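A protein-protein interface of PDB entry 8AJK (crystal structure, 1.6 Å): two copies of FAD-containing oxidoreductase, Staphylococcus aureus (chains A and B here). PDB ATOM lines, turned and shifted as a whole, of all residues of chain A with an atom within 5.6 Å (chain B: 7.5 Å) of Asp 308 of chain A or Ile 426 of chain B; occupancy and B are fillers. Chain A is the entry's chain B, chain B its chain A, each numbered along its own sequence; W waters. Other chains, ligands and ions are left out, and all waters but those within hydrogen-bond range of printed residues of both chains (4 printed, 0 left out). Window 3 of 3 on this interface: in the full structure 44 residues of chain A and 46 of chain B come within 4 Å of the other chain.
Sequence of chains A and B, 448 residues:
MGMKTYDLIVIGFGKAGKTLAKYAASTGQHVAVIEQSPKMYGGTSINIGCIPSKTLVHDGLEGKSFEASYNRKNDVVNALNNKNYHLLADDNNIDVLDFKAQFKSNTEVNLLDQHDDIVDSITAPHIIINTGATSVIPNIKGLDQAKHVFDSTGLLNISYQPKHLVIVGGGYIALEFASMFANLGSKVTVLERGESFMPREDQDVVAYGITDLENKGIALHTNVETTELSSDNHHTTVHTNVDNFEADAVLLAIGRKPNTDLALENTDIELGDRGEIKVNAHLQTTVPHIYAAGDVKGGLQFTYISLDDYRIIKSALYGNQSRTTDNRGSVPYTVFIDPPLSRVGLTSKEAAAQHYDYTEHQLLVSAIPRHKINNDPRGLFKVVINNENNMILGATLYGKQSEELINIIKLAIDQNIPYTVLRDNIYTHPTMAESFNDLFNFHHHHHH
ND2 of Asn 407 of chain A is in hydrogen-bond range of OG1 of Thr 428 of chain B (3.1 Å).
The guanidinium group of Arg 311 of chain A lies close to the backbone carbonyl oxygen of Asp 424 of chain B, 3.4 Å away.
The backbone carbonyl oxygen (O) of Asn 425 of chain B is in hydrogen-bond range of the guanidinium group (NH2) of Arg 311 of chain A.
ND2 of Asn 437 of chain B lies close to NH2 of Arg 311 of chain A, at 3.2 Å.
OD2 of Asp 308 of chain A lies within salt-bridge range of NH1 of Arg 328 of chain A (2.8 Å).
The side-chain amide nitrogen of Asn 437 of chain B lies within hydrogen-bond range of the backbone carbonyl oxygen of Arg 423 of chain B (2.9 Å).
OH of Tyr 304 of chain A is in hydrogen-bond range of O of Pro 332 of chain A (2.7 Å).
The guanidinium group of Arg 423 of chain B lies within salt-bridge range of the side-chain carboxylate of Asp 424 of chain B (2.8 Å).
ND2 of Asn 437 of chain B is in hydrogen-bond range of O of Asn 425 of chain B.
The side-chain amide oxygen of Asn 425 of chain B lies close to the backbone carbonyl oxygen of Val 421 of chain B, 3.5 Å away.
Ile 426 of chain B touches Tyr 304 of chain A.
Tyr 427 of chain B touches Tyr 304 of chain A (O to CG, 3.2 Å).
Thr 428 of chain B touches Tyr 304 of chain A (CA to CE2, 3.9 Å).
CD2 of Leu 307 of chain A touches OD1 of Asn 437 of chain B, 3.7 Å away.
CG of Asp 308 of chain A touches CD1 of Ile 426 of chain B, 3.7 Å away.
Ile 426 of chain B touches Arg 328 of chain A (CD1 to O, 3.7 Å).
Pro 332 of chain A touches Thr 428 of chain B (CG to CG2, 3.8 Å).
Asn 407 of chain A touches Tyr 427 of chain B (OD1 to CA, 3.4 Å).
Asn 425 of chain B touches Lys 410 of chain A.
Ile 426 of chain B touches Lys 410 of chain A.
Of chain B, only Ile 426 comes within 4 Å of Asp 308 of chain A.
Of the printed residues of chain B, Arg 311 of chain A touches Asp 424, Asn 425 and Asn 437.
Of the printed residues of chain B, Arg 328 of chain A touches Ile 426.
Ser 330 of chain A touches none of the printed residues of chain B.
Printed residues of chain B within 4 Å of Lys 410 of chain A: Asn 425 and Ile 426.
Val 421 of chain B touches none of the printed residues of chain A.
Printed residues of chain A within 4 Å of Asn 425 of chain B: Arg 311 and Lys 410.
Ile 426 of chain B touches just these residues of chain A: Tyr 304 (3.3 Å), Asp 308 (3.7 Å), Arg 328 (3.7 Å) and Lys 410 (3.3 Å).
Of the printed residues of chain A, Thr 428 of chain B touches Tyr 304 (3.9 Å), Pro 332 (3.8 Å) and Asn 407 (3.1 Å).
The nearest residue of chain B that does not touch Asp 308 of chain A is Asp 424 of chain B (4.8 Å).
Of the 20 printed residues of chain A, 8 touch a printed residue of chain B.
Printed residues of chain A that touch a printed residue of chain B: Tyr 304, Leu 307, Asp 308, Arg 311, Arg 328, Pro 332, Asn 407 and Lys 410.
Among the printed residues, 14 pairs touch across the chains.
No position is printed for both chains.
Water W2 bridges the backbone carbonyl oxygen (O) of Ile 426 of chain B (2.7 Å) and the side-chain amide oxygen (OD1) of Asn 407 of chain A (2.7 Å).
Water W3 lies within hydrogen-bond range of NZ of Lys 410 of chain A (2.8 Å), O of Arg 328 of chain A (3.0 Å), N of Ile 426 of chain B (3.0 Å) and OD1 of Asn 425 of chain B (3.1 Å).
Water W4 lies within hydrogen-bond range of OD1 of Asp 424 of chain B (2.8 Å) and NE of Arg 311 of chain A (3.1 Å).
Water W1 lies within hydrogen-bond range of the guanidinium group of Arg 311 of chain A (3.1 Å) and the backbone carbonyl oxygen of Arg 423 of chain B (3.4 Å).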
ATOM      1  N   THR A 303      -6.223 -25.109  -9.834  1.00  0.00           N
ATOM      2  CA  THR A 303      -6.002 -23.983 -10.736  1.00  0.00           C
ATOM      3  C   THR A 303      -5.895 -22.667  -9.972  1.00  0.00           C
ATOM      4  O   THR A 303      -5.078 -21.803 -10.328  1.00  0.00           O
ATOM      5  CB  THR A 303      -7.136 -23.944 -11.768  1.00  0.00           C
ATOM      6  OG1 THR A 303      -7.118 -25.179 -12.497  1.00  0.00           O
ATOM      7  CG2 THR A 303      -6.931 -22.800 -12.754  1.00  0.00           C
ATOM      8  N   TYR A 304      -6.640 -22.536  -8.882  1.00  0.00           N
ATOM      9  CA  TYR A 304      -6.622 -21.301  -8.119  1.00  0.00           C
ATOM     10  C   TYR A 304      -5.423 -21.212  -7.186  1.00  0.00           C
ATOM     11  O   TYR A 304      -5.106 -20.114  -6.726  1.00  0.00           O
ATOM     12  CB  TYR A 304      -7.916 -21.143  -7.310  1.00  0.00           C
ATOM     13  CG  TYR A 304      -8.397 -22.393  -6.600  1.00  0.00           C
ATOM     14  CD1 TYR A 304      -7.973 -22.688  -5.307  1.00  0.00           C
ATOM     15  CD2 TYR A 304      -9.295 -23.264  -7.214  1.00  0.00           C
ATOM     16  CE1 TYR A 304      -8.429 -23.821  -4.642  1.00  0.00           C
ATOM     17  CE2 TYR A 304      -9.765 -24.387  -6.559  1.00  0.00           C
ATOM     18  CZ  TYR A 304      -9.333 -24.666  -5.283  1.00  0.00           C
ATOM     19  OH  TYR A 304      -9.825 -25.786  -4.652  1.00  0.00           O
ATOM     20  N   ILE A 305      -4.760 -22.336  -6.886  1.00  0.00           N
ATOM     21  CA  ILE A 305      -3.476 -22.243  -6.194  1.00  0.00           C
ATOM     22  C   ILE A 305      -2.421 -21.722  -7.149  1.00  0.00           C
ATOM     23  O   ILE A 305      -1.587 -20.884  -6.781  1.00  0.00           O
ATOM     24  CB  ILE A 305      -3.083 -23.603  -5.587  1.00  0.00           C
ATOM     25  CG1 ILE A 305      -3.961 -23.905  -4.367  1.00  0.00           C
ATOM     26  CG2 ILE A 305      -1.585 -23.643  -5.214  1.00  0.00           C
ATOM     27  CD1 ILE A 305      -3.601 -23.058  -3.148  1.00  0.00           C
ATOM     28  N   SER A 306      -2.437 -22.218  -8.397  1.00  0.00           N
ATOM     29  CA  SER A 306      -1.553 -21.655  -9.414  1.00  0.00           C
ATOM     30  C   SER A 306      -1.811 -20.163  -9.599  1.00  0.00           C
ATOM     31  O   SER A 306      -0.866 -19.370  -9.720  1.00  0.00           O
ATOM     32  CB  SER A 306      -1.726 -22.401 -10.739  1.00  0.00           C
ATOM     33  OG  SER A 306      -0.669 -22.048 -11.636  1.00  0.00           O
ATOM     34  N   LEU A 307      -3.083 -19.761  -9.635  1.00  0.00           N
ATOM     35  CA  LEU A 307      -3.384 -18.335  -9.743  1.00  0.00           C
ATOM     36  C   LEU A 307      -2.830 -17.573  -8.547  1.00  0.00           C
ATOM     37  O   LEU A 307      -2.252 -16.487  -8.699  1.00  0.00           O
ATOM     38  CB  LEU A 307      -4.895 -18.121  -9.873  1.00  0.00           C
ATOM     39  CG  LEU A 307      -5.309 -16.646  -9.907  1.00  0.00           C
ATOM     40  CD1 LEU A 307      -4.604 -15.920 -11.049  1.00  0.00           C
ATOM     41  CD2 LEU A 307      -6.835 -16.553 -10.053  1.00  0.00           C
ATOM     42  N   ASP A 308      -2.966 -18.138  -7.347  1.00  0.00           N
ATOM     43  CA  ASP A 308      -2.405 -17.457  -6.190  1.00  0.00           C
ATOM     44  C   ASP A 308      -0.889 -17.406  -6.235  1.00  0.00           C
ATOM     45  O   ASP A 308      -0.290 -16.439  -5.746  1.00  0.00           O
ATOM     46  CB  ASP A 308      -2.866 -18.122  -4.902  1.00  0.00           C
ATOM     47  CG  ASP A 308      -2.612 -17.240  -3.693  1.00  0.00           C
ATOM     48  OD1 ASP A 308      -3.126 -16.096  -3.679  1.00  0.00           O
ATOM     49  OD2 ASP A 308      -1.904 -17.687  -2.763  1.00  0.00           O
ATOM     50  N   ASP A 309      -0.250 -18.427  -6.816  1.00  0.00           N
ATOM     51  CA  ASP A 309       1.194 -18.410  -6.994  1.00  0.00           C
ATOM     52  C   ASP A 309       1.631 -17.229  -7.851  1.00  0.00           C
ATOM     53  O   ASP A 309       2.694 -16.638  -7.615  1.00  0.00           O
ATOM     54  CB  ASP A 309       1.666 -19.727  -7.634  1.00  0.00           C
ATOM     55  CG  ASP A 309       1.539 -20.923  -6.712  1.00  0.00           C
ATOM     56  OD1 ASP A 309       1.382 -20.751  -5.483  1.00  0.00           O
ATOM     57  OD2 ASP A 309       1.631 -22.065  -7.220  1.00  0.00           O
ATOM     58  N   TYR A 310       0.829 -16.871  -8.858  1.00  0.00           N
ATOM     59  CA  TYR A 310       1.122 -15.658  -9.615  1.00  0.00           C
ATOM     60  C   TYR A 310       1.109 -14.436  -8.706  1.00  0.00           C
ATOM     61  O   TYR A 310       1.962 -13.548  -8.845  1.00  0.00           O
ATOM     62  CB  TYR A 310       0.125 -15.487 -10.765  1.00  0.00           C
ATOM     63  CG  TYR A 310      -0.312 -14.059 -11.031  1.00  0.00           C
ATOM     64  CD1 TYR A 310       0.463 -13.200 -11.801  1.00  0.00           C
ATOM     65  CD2 TYR A 310      -1.506 -13.582 -10.512  1.00  0.00           C
ATOM     66  CE1 TYR A 310       0.064 -11.888 -12.046  1.00  0.00           C
ATOM     67  CE2 TYR A 310      -1.917 -12.260 -10.739  1.00  0.00           C
ATOM     68  CZ  TYR A 310      -1.132 -11.433 -11.518  1.00  0.00           C
ATOM     69  OH  TYR A 310      -1.534 -10.134 -11.755  1.00  0.00           O
ATOM     70  N   ARG A 311       0.159 -14.375  -7.763  1.00  0.00           N
ATOM     71  CA  ARG A 311       0.115 -13.237  -6.843  1.00  0.00           C
ATOM     72  C   ARG A 311       1.385 -13.164  -6.000  1.00  0.00           C
ATOM     73  O   ARG A 311       1.916 -12.072  -5.751  1.00  0.00           O
ATOM     74  CB  ARG A 311      -1.112 -13.339  -5.942  1.00  0.00           C
ATOM     75  CG  ARG A 311      -2.465 -13.354  -6.694  1.00  0.00           C
ATOM     76  CD  ARG A 311      -3.643 -13.074  -5.764  1.00  0.00           C
ATOM     77  NE  ARG A 311      -4.918 -13.256  -6.461  1.00  0.00           N
ATOM     78  CZ  ARG A 311      -5.607 -14.391  -6.494  1.00  0.00           C
ATOM     79  NH1 ARG A 311      -5.225 -15.462  -5.807  1.00  0.00           N
ATOM     80  NH2 ARG A 311      -6.711 -14.462  -7.242  1.00  0.00           N
ATOM     81  N   ILE A 312       1.881 -14.321  -5.551  1.00  0.00           N
ATOM     82  CA  ILE A 312       3.097 -14.376  -4.743  1.00  0.00           C
ATOM     83  C   ILE A 312       4.303 -13.949  -5.560  1.00  0.00           C
ATOM     84  O   ILE A 312       5.149 -13.170  -5.097  1.00  0.00           O
ATOM     85  CB  ILE A 312       3.278 -15.795  -4.168  1.00  0.00           C
ATOM     86  CG1 ILE A 312       2.122 -16.116  -3.220  1.00  0.00           C
ATOM     87  CG2 ILE A 312       4.669 -15.956  -3.476  1.00  0.00           C
ATOM     88  CD1 ILE A 312       1.987 -17.601  -2.889  1.00  0.00           C
ATOM     89  N   ILE A 313       4.415 -14.464  -6.783  1.00  0.00           N
ATOM     90  CA  ILE A 313       5.585 -14.161  -7.601  1.00  0.00           C
ATOM     91  C   ILE A 313       5.537 -12.716  -8.075  1.00  0.00           C
ATOM     92  O   ILE A 313       6.564 -12.026  -8.100  1.00  0.00           O
ATOM     93  CB  ILE A 313       5.690 -15.162  -8.768  1.00  0.00           C
ATOM     94  CG1 ILE A 313       6.026 -16.556  -8.231  1.00  0.00           C
ATOM     95  CG2 ILE A 313       6.756 -14.720  -9.786  1.00  0.00           C
ATOM     96  CD1 ILE A 313       5.933 -17.674  -9.280  1.00  0.00           C
ATOM     97  N   ARG A 323       3.370 -11.105   0.029  1.00  0.00           N
ATOM     98  CA  ARG A 323       2.580 -12.310  -0.209  1.00  0.00           C
ATOM     99  C   ARG A 323       3.498 -13.529  -0.208  1.00  0.00           C
ATOM    100  O   ARG A 323       4.533 -13.521  -0.882  1.00  0.00           O
ATOM    101  CB  ARG A 323       1.836 -12.221  -1.543  1.00  0.00           C
ATOM    102  CG  ARG A 323       0.430 -11.598  -1.477  1.00  0.00           C
ATOM    103  CD  ARG A 323      -0.431 -12.178  -0.346  1.00  0.00           C
ATOM    104  NE  ARG A 323      -0.334 -13.630  -0.269  1.00  0.00           N
ATOM    105  CZ  ARG A 323      -0.852 -14.465  -1.160  1.00  0.00           C
ATOM    106  NH1 ARG A 323      -1.551 -14.027  -2.192  1.00  0.00           N
ATOM    107  NH2 ARG A 323      -0.659 -15.774  -1.012  1.00  0.00           N
ATOM    108  N   THR A 324       3.119 -14.573   0.544  1.00  0.00           N
ATOM    109  CA  THR A 324       3.882 -15.825   0.579  1.00  0.00           C
ATOM    110  C   THR A 324       2.918 -17.005   0.545  1.00  0.00           C
ATOM    111  O   THR A 324       1.695 -16.851   0.606  1.00  0.00           O
ATOM    112  CB  THR A 324       4.736 -15.964   1.846  1.00  0.00           C
ATOM    113  OG1 THR A 324       3.866 -16.097   2.977  1.00  0.00           O
ATOM    114  CG2 THR A 324       5.619 -14.728   2.052  1.00  0.00           C
ATOM    115  N   ARG A 328      -1.851 -17.323   2.323  1.00  0.00           N
ATOM    116  CA  ARG A 328      -2.847 -17.467   1.271  1.00  0.00           C
ATOM    117  C   ARG A 328      -4.267 -17.250   1.772  1.00  0.00           C
ATOM    118  O   ARG A 328      -5.149 -16.968   0.959  1.00  0.00           O
ATOM    119  CB  ARG A 328      -2.791 -18.869   0.658  1.00  0.00           C
ATOM    120  CG  ARG A 328      -1.460 -19.266   0.005  1.00  0.00           C
ATOM    121  CD  ARG A 328      -1.733 -20.556  -0.801  1.00  0.00           C
ATOM    122  NE  ARG A 328      -0.545 -21.224  -1.323  1.00  0.00           N
ATOM    123  CZ  ARG A 328      -0.023 -21.014  -2.527  1.00  0.00           C
ATOM    124  NH1 ARG A 328      -0.470 -20.049  -3.317  1.00  0.00           N
ATOM    125  NH2 ARG A 328       0.972 -21.795  -2.948  1.00  0.00           N
ATOM    126  N   GLY A 329      -4.511 -17.405   3.076  1.00  0.00           N
ATOM    127  CA  GLY A 329      -5.867 -17.531   3.578  1.00  0.00           C
ATOM    128  C   GLY A 329      -6.334 -18.972   3.476  1.00  0.00           C
ATOM    129  O   GLY A 329      -5.622 -19.856   3.000  1.00  0.00           O
ATOM    130  N   SER A 330      -7.571 -19.217   3.911  1.00  0.00           N
ATOM    131  CA  SER A 330      -8.099 -20.577   3.883  1.00  0.00           C
ATOM    132  C   SER A 330      -8.324 -21.043   2.440  1.00  0.00           C
ATOM    133  O   SER A 330      -8.765 -20.274   1.584  1.00  0.00           O
ATOM    134  CB  SER A 330      -9.406 -20.637   4.689  1.00  0.00           C
ATOM    135  OG  SER A 330     -10.345 -19.704   4.196  1.00  0.00           O
ATOM    136  N   VAL A 331      -7.986 -22.301   2.158  1.00  0.00           N
ATOM    137  CA  VAL A 331      -8.035 -22.800   0.790  1.00  0.00           C
ATOM    138  C   VAL A 331      -9.242 -23.731   0.667  1.00  0.00           C
ATOM    139  O   VAL A 331      -9.223 -24.854   1.198  1.00  0.00           O
ATOM    140  CB  VAL A 331      -6.737 -23.517   0.393  1.00  0.00           C
ATOM    141  CG1 VAL A 331      -6.828 -24.013  -1.050  1.00  0.00           C
ATOM    142  CG2 VAL A 331      -5.539 -22.583   0.569  1.00  0.00           C
ATOM    143  N   PRO A 332     -10.303 -23.314  -0.010  1.00  0.00           N
ATOM    144  CA  PRO A 332     -11.477 -24.175  -0.161  1.00  0.00           C
ATOM    145  C   PRO A 332     -11.268 -25.126  -1.316  1.00  0.00           C
ATOM    146  O   PRO A 332     -10.387 -24.930  -2.153  1.00  0.00           O
ATOM    147  CB  PRO A 332     -12.596 -23.178  -0.483  1.00  0.00           C
ATOM    148  CG  PRO A 332     -11.868 -22.163  -1.357  1.00  0.00           C
ATOM    149  CD  PRO A 332     -10.493 -22.014  -0.690  1.00  0.00           C
ATOM    150  N   ASN A 407     -17.505 -20.479  -0.765  1.00  0.00           N
ATOM    151  CA  ASN A 407     -16.747 -19.236  -0.790  1.00  0.00           C
ATOM    152  C   ASN A 407     -17.231 -18.232   0.256  1.00  0.00           C
ATOM    153  O   ASN A 407     -16.445 -17.386   0.699  1.00  0.00           O
ATOM    154  CB  ASN A 407     -16.810 -18.632  -2.199  1.00  0.00           C
ATOM    155  CG  ASN A 407     -16.156 -19.533  -3.234  1.00  0.00           C
ATOM    156  OD1 ASN A 407     -14.931 -19.671  -3.257  1.00  0.00           O
ATOM    157  ND2 ASN A 407     -16.974 -20.185  -4.078  1.00  0.00           N
ATOM    158  N   LYS A 410     -15.356 -19.491   3.392  1.00  0.00           N
ATOM    159  CA  LYS A 410     -13.949 -19.096   3.269  1.00  0.00           C
ATOM    160  C   LYS A 410     -13.749 -17.632   3.652  1.00  0.00           C
ATOM    161  O   LYS A 410     -12.831 -17.290   4.413  1.00  0.00           O
ATOM    162  CB  LYS A 410     -13.457 -19.346   1.831  1.00  0.00           C
ATOM    163  CG  LYS A 410     -11.973 -18.995   1.530  1.00  0.00           C
ATOM    164  CD  LYS A 410     -11.767 -17.480   1.231  1.00  0.00           C
ATOM    165  CE  LYS A 410     -10.482 -17.225   0.443  1.00  0.00           C
ATOM    166  NZ  LYS A 410      -9.245 -17.569   1.219  1.00  0.00           N
ATOM    167  N   VAL B 421     -10.187  -7.074  -1.224  1.00  0.00           N
ATOM    168  CA  VAL B 421     -10.154  -8.419  -0.650  1.00  0.00           C
ATOM    169  C   VAL B 421     -10.881  -9.400  -1.568  1.00  0.00           C
ATOM    170  O   VAL B 421     -10.412 -10.524  -1.810  1.00  0.00           O
ATOM    171  CB  VAL B 421     -10.773  -8.412   0.763  1.00  0.00           C
ATOM    172  CG1 VAL B 421     -10.987  -9.835   1.280  1.00  0.00           C
ATOM    173  CG2 VAL B 421      -9.920  -7.591   1.737  1.00  0.00           C
ATOM    174  N   LEU B 422     -12.031  -8.992  -2.104  1.00  0.00           N
ATOM    175  CA  LEU B 422     -12.755  -9.856  -3.033  1.00  0.00           C
ATOM    176  C   LEU B 422     -12.013  -9.983  -4.357  1.00  0.00           C
ATOM    177  O   LEU B 422     -12.078 -11.037  -5.012  1.00  0.00           O
ATOM    178  CB  LEU B 422     -14.177  -9.308  -3.246  1.00  0.00           C
ATOM    179  CG  LEU B 422     -15.197  -9.642  -2.155  1.00  0.00           C
ATOM    180  CD1 LEU B 422     -14.834  -9.094  -0.804  1.00  0.00           C
ATOM    181  CD2 LEU B 422     -16.595  -9.127  -2.568  1.00  0.00           C
ATOM    182  N   ARG B 423     -11.271  -8.944  -4.751  1.00  0.00           N
ATOM    183  CA  ARG B 423     -10.460  -9.030  -5.961  1.00  0.00           C
ATOM    184  C   ARG B 423      -9.364 -10.089  -5.822  1.00  0.00           C
ATOM    185  O   ARG B 423      -9.082 -10.842  -6.763  1.00  0.00           O
ATOM    186  CB  ARG B 423      -9.802  -7.677  -6.259  1.00  0.00           C
ATOM    187  CG  ARG B 423      -8.882  -7.739  -7.487  1.00  0.00           C
ATOM    188  CD  ARG B 423      -7.994  -6.498  -7.585  1.00  0.00           C
ATOM    189  NE  ARG B 423      -7.130  -6.383  -6.414  1.00  0.00           N
ATOM    190  CZ  ARG B 423      -6.607  -5.249  -5.964  1.00  0.00           C
ATOM    191  NH1 ARG B 423      -6.822  -4.093  -6.576  1.00  0.00           N
ATOM    192  NH2 ARG B 423      -5.833  -5.280  -4.881  1.00  0.00           N
ATOM    193  N   ASP B 424      -8.729 -10.147  -4.660  1.00  0.00           N
ATOM    194  CA  ASP B 424      -7.514 -10.941  -4.493  1.00  0.00           C
ATOM    195  C   ASP B 424      -7.765 -12.325  -3.891  1.00  0.00           C
ATOM    196  O   ASP B 424      -6.806 -13.086  -3.693  1.00  0.00           O
ATOM    197  CB  ASP B 424      -6.511 -10.174  -3.630  1.00  0.00           C
ATOM    198  CG  ASP B 424      -5.986  -8.906  -4.307  1.00  0.00           C
ATOM    199  OD1 ASP B 424      -6.002  -8.813  -5.556  1.00  0.00           O
ATOM    200  OD2 ASP B 424      -5.536  -7.999  -3.585  1.00  0.00           O
ATOM    201  N   ASN B 425      -9.012 -12.675  -3.597  1.00  0.00           N
ATOM    202  CA  ASN B 425      -9.260 -13.902  -2.858  1.00  0.00           C
ATOM    203  C   ASN B 425      -9.109 -15.146  -3.732  1.00  0.00           C
ATOM    204  O   ASN B 425      -9.231 -15.107  -4.957  1.00  0.00           O
ATOM    205  CB  ASN B 425     -10.660 -13.889  -2.221  1.00  0.00           C
ATOM    206  CG  ASN B 425     -10.604 -13.501  -0.747  1.00  0.00           C
ATOM    207  OD1 ASN B 425      -9.523 -13.446  -0.159  1.00  0.00           O
ATOM    208  ND2 ASN B 425     -11.754 -13.287  -0.140  1.00  0.00           N
ATOM    209  N   ILE B 426      -8.837 -16.260  -3.060  1.00  0.00           N
ATOM    210  CA  ILE B 426      -8.847 -17.582  -3.681  1.00  0.00           C
ATOM    211  C   ILE B 426     -10.290 -18.078  -3.711  1.00  0.00           C
ATOM    212  O   ILE B 426     -10.943 -18.165  -2.665  1.00  0.00           O
ATOM    213  CB  ILE B 426      -7.953 -18.542  -2.895  1.00  0.00           C
ATOM    214  CG1 ILE B 426      -6.492 -18.153  -3.081  1.00  0.00           C
ATOM    215  CG2 ILE B 426      -8.167 -19.982  -3.377  1.00  0.00           C
ATOM    216  CD1 ILE B 426      -5.492 -18.914  -2.168  1.00  0.00           C
ATOM    217  N   TYR B 427     -10.794 -18.401  -4.905  1.00  0.00           N
ATOM    218  CA  TYR B 427     -12.136 -18.943  -5.081  1.00  0.00           C
ATOM    219  C   TYR B 427     -12.068 -20.351  -5.649  1.00  0.00           C
ATOM    220  O   TYR B 427     -11.104 -20.707  -6.338  1.00  0.00           O
ATOM    221  CB  TYR B 427     -12.980 -18.106  -6.037  1.00  0.00           C
ATOM    222  CG  TYR B 427     -13.239 -16.695  -5.557  1.00  0.00           C
ATOM    223  CD1 TYR B 427     -12.373 -15.656  -5.883  1.00  0.00           C
ATOM    224  CD2 TYR B 427     -14.328 -16.425  -4.744  1.00  0.00           C
ATOM    225  CE1 TYR B 427     -12.621 -14.359  -5.429  1.00  0.00           C
ATOM    226  CE2 TYR B 427     -14.577 -15.136  -4.292  1.00  0.00           C
ATOM    227  CZ  TYR B 427     -13.717 -14.121  -4.632  1.00  0.00           C
ATOM    228  OH  TYR B 427     -13.953 -12.837  -4.164  1.00  0.00           O
ATOM    229  N   THR B 428     -13.105 -21.151  -5.391  1.00  0.00           N
ATOM    230  CA  THR B 428     -13.149 -22.459  -6.040  1.00  0.00           C
ATOM    231  C   THR B 428     -13.292 -22.278  -7.551  1.00  0.00           C
ATOM    232  O   THR B 428     -13.631 -21.205  -8.046  1.00  0.00           O
ATOM    233  CB  THR B 428     -14.303 -23.307  -5.504  1.00  0.00           C
ATOM    234  OG1 THR B 428     -15.463 -22.485  -5.428  1.00  0.00           O
ATOM    235  CG2 THR B 428     -13.981 -23.837  -4.104  1.00  0.00           C
ATOM    236  N   GLU B 434     -15.626 -17.304  -8.862  1.00  0.00           N
ATOM    237  CA  GLU B 434     -14.266 -16.858  -9.146  1.00  0.00           C
ATOM    238  C   GLU B 434     -14.214 -15.701 -10.136  1.00  0.00           C
ATOM    239  O   GLU B 434     -13.148 -15.093 -10.293  1.00  0.00           O
ATOM    240  CB  GLU B 434     -13.399 -18.010  -9.688  1.00  0.00           C
ATOM    241  CG  GLU B 434     -13.927 -18.580 -10.966  1.00  0.00           C
ATOM    242  CD  GLU B 434     -13.099 -19.737 -11.471  1.00  0.00           C
ATOM    243  OE1 GLU B 434     -11.862 -19.769 -11.236  1.00  0.00           O
ATOM    244  OE2 GLU B 434     -13.718 -20.650 -12.048  1.00  0.00           O
ATOM    245  N   ASN B 437     -12.548 -12.350  -9.123  1.00  0.00           N
ATOM    246  CA  ASN B 437     -11.158 -11.960  -9.362  1.00  0.00           C
ATOM    247  C   ASN B 437     -11.050 -10.956 -10.497  1.00  0.00           C
ATOM    248  O   ASN B 437     -10.115 -10.153 -10.523  1.00  0.00           O
ATOM    249  CB  ASN B 437     -10.265 -13.176  -9.710  1.00  0.00           C
ATOM    250  CG  ASN B 437     -10.052 -14.145  -8.544  1.00  0.00           C
ATOM    251  OD1 ASN B 437     -10.033 -15.369  -8.746  1.00  0.00           O
ATOM    252  ND2 ASN B 437      -9.826 -13.615  -7.348  1.00  0.00           N
HETATM  253  O   HOH W   1      -6.896 -11.999  -9.063  1.00  0.00           O
HETATM  254  O   HOH W   2     -13.401 -18.244  -1.523  1.00  0.00           O
HETATM  255  O   HOH W   3      -7.583 -15.914  -0.348  1.00  0.00           O
HETATM  256  O   HOH W   4      -5.171 -10.421  -7.757  1.00  0.00           O
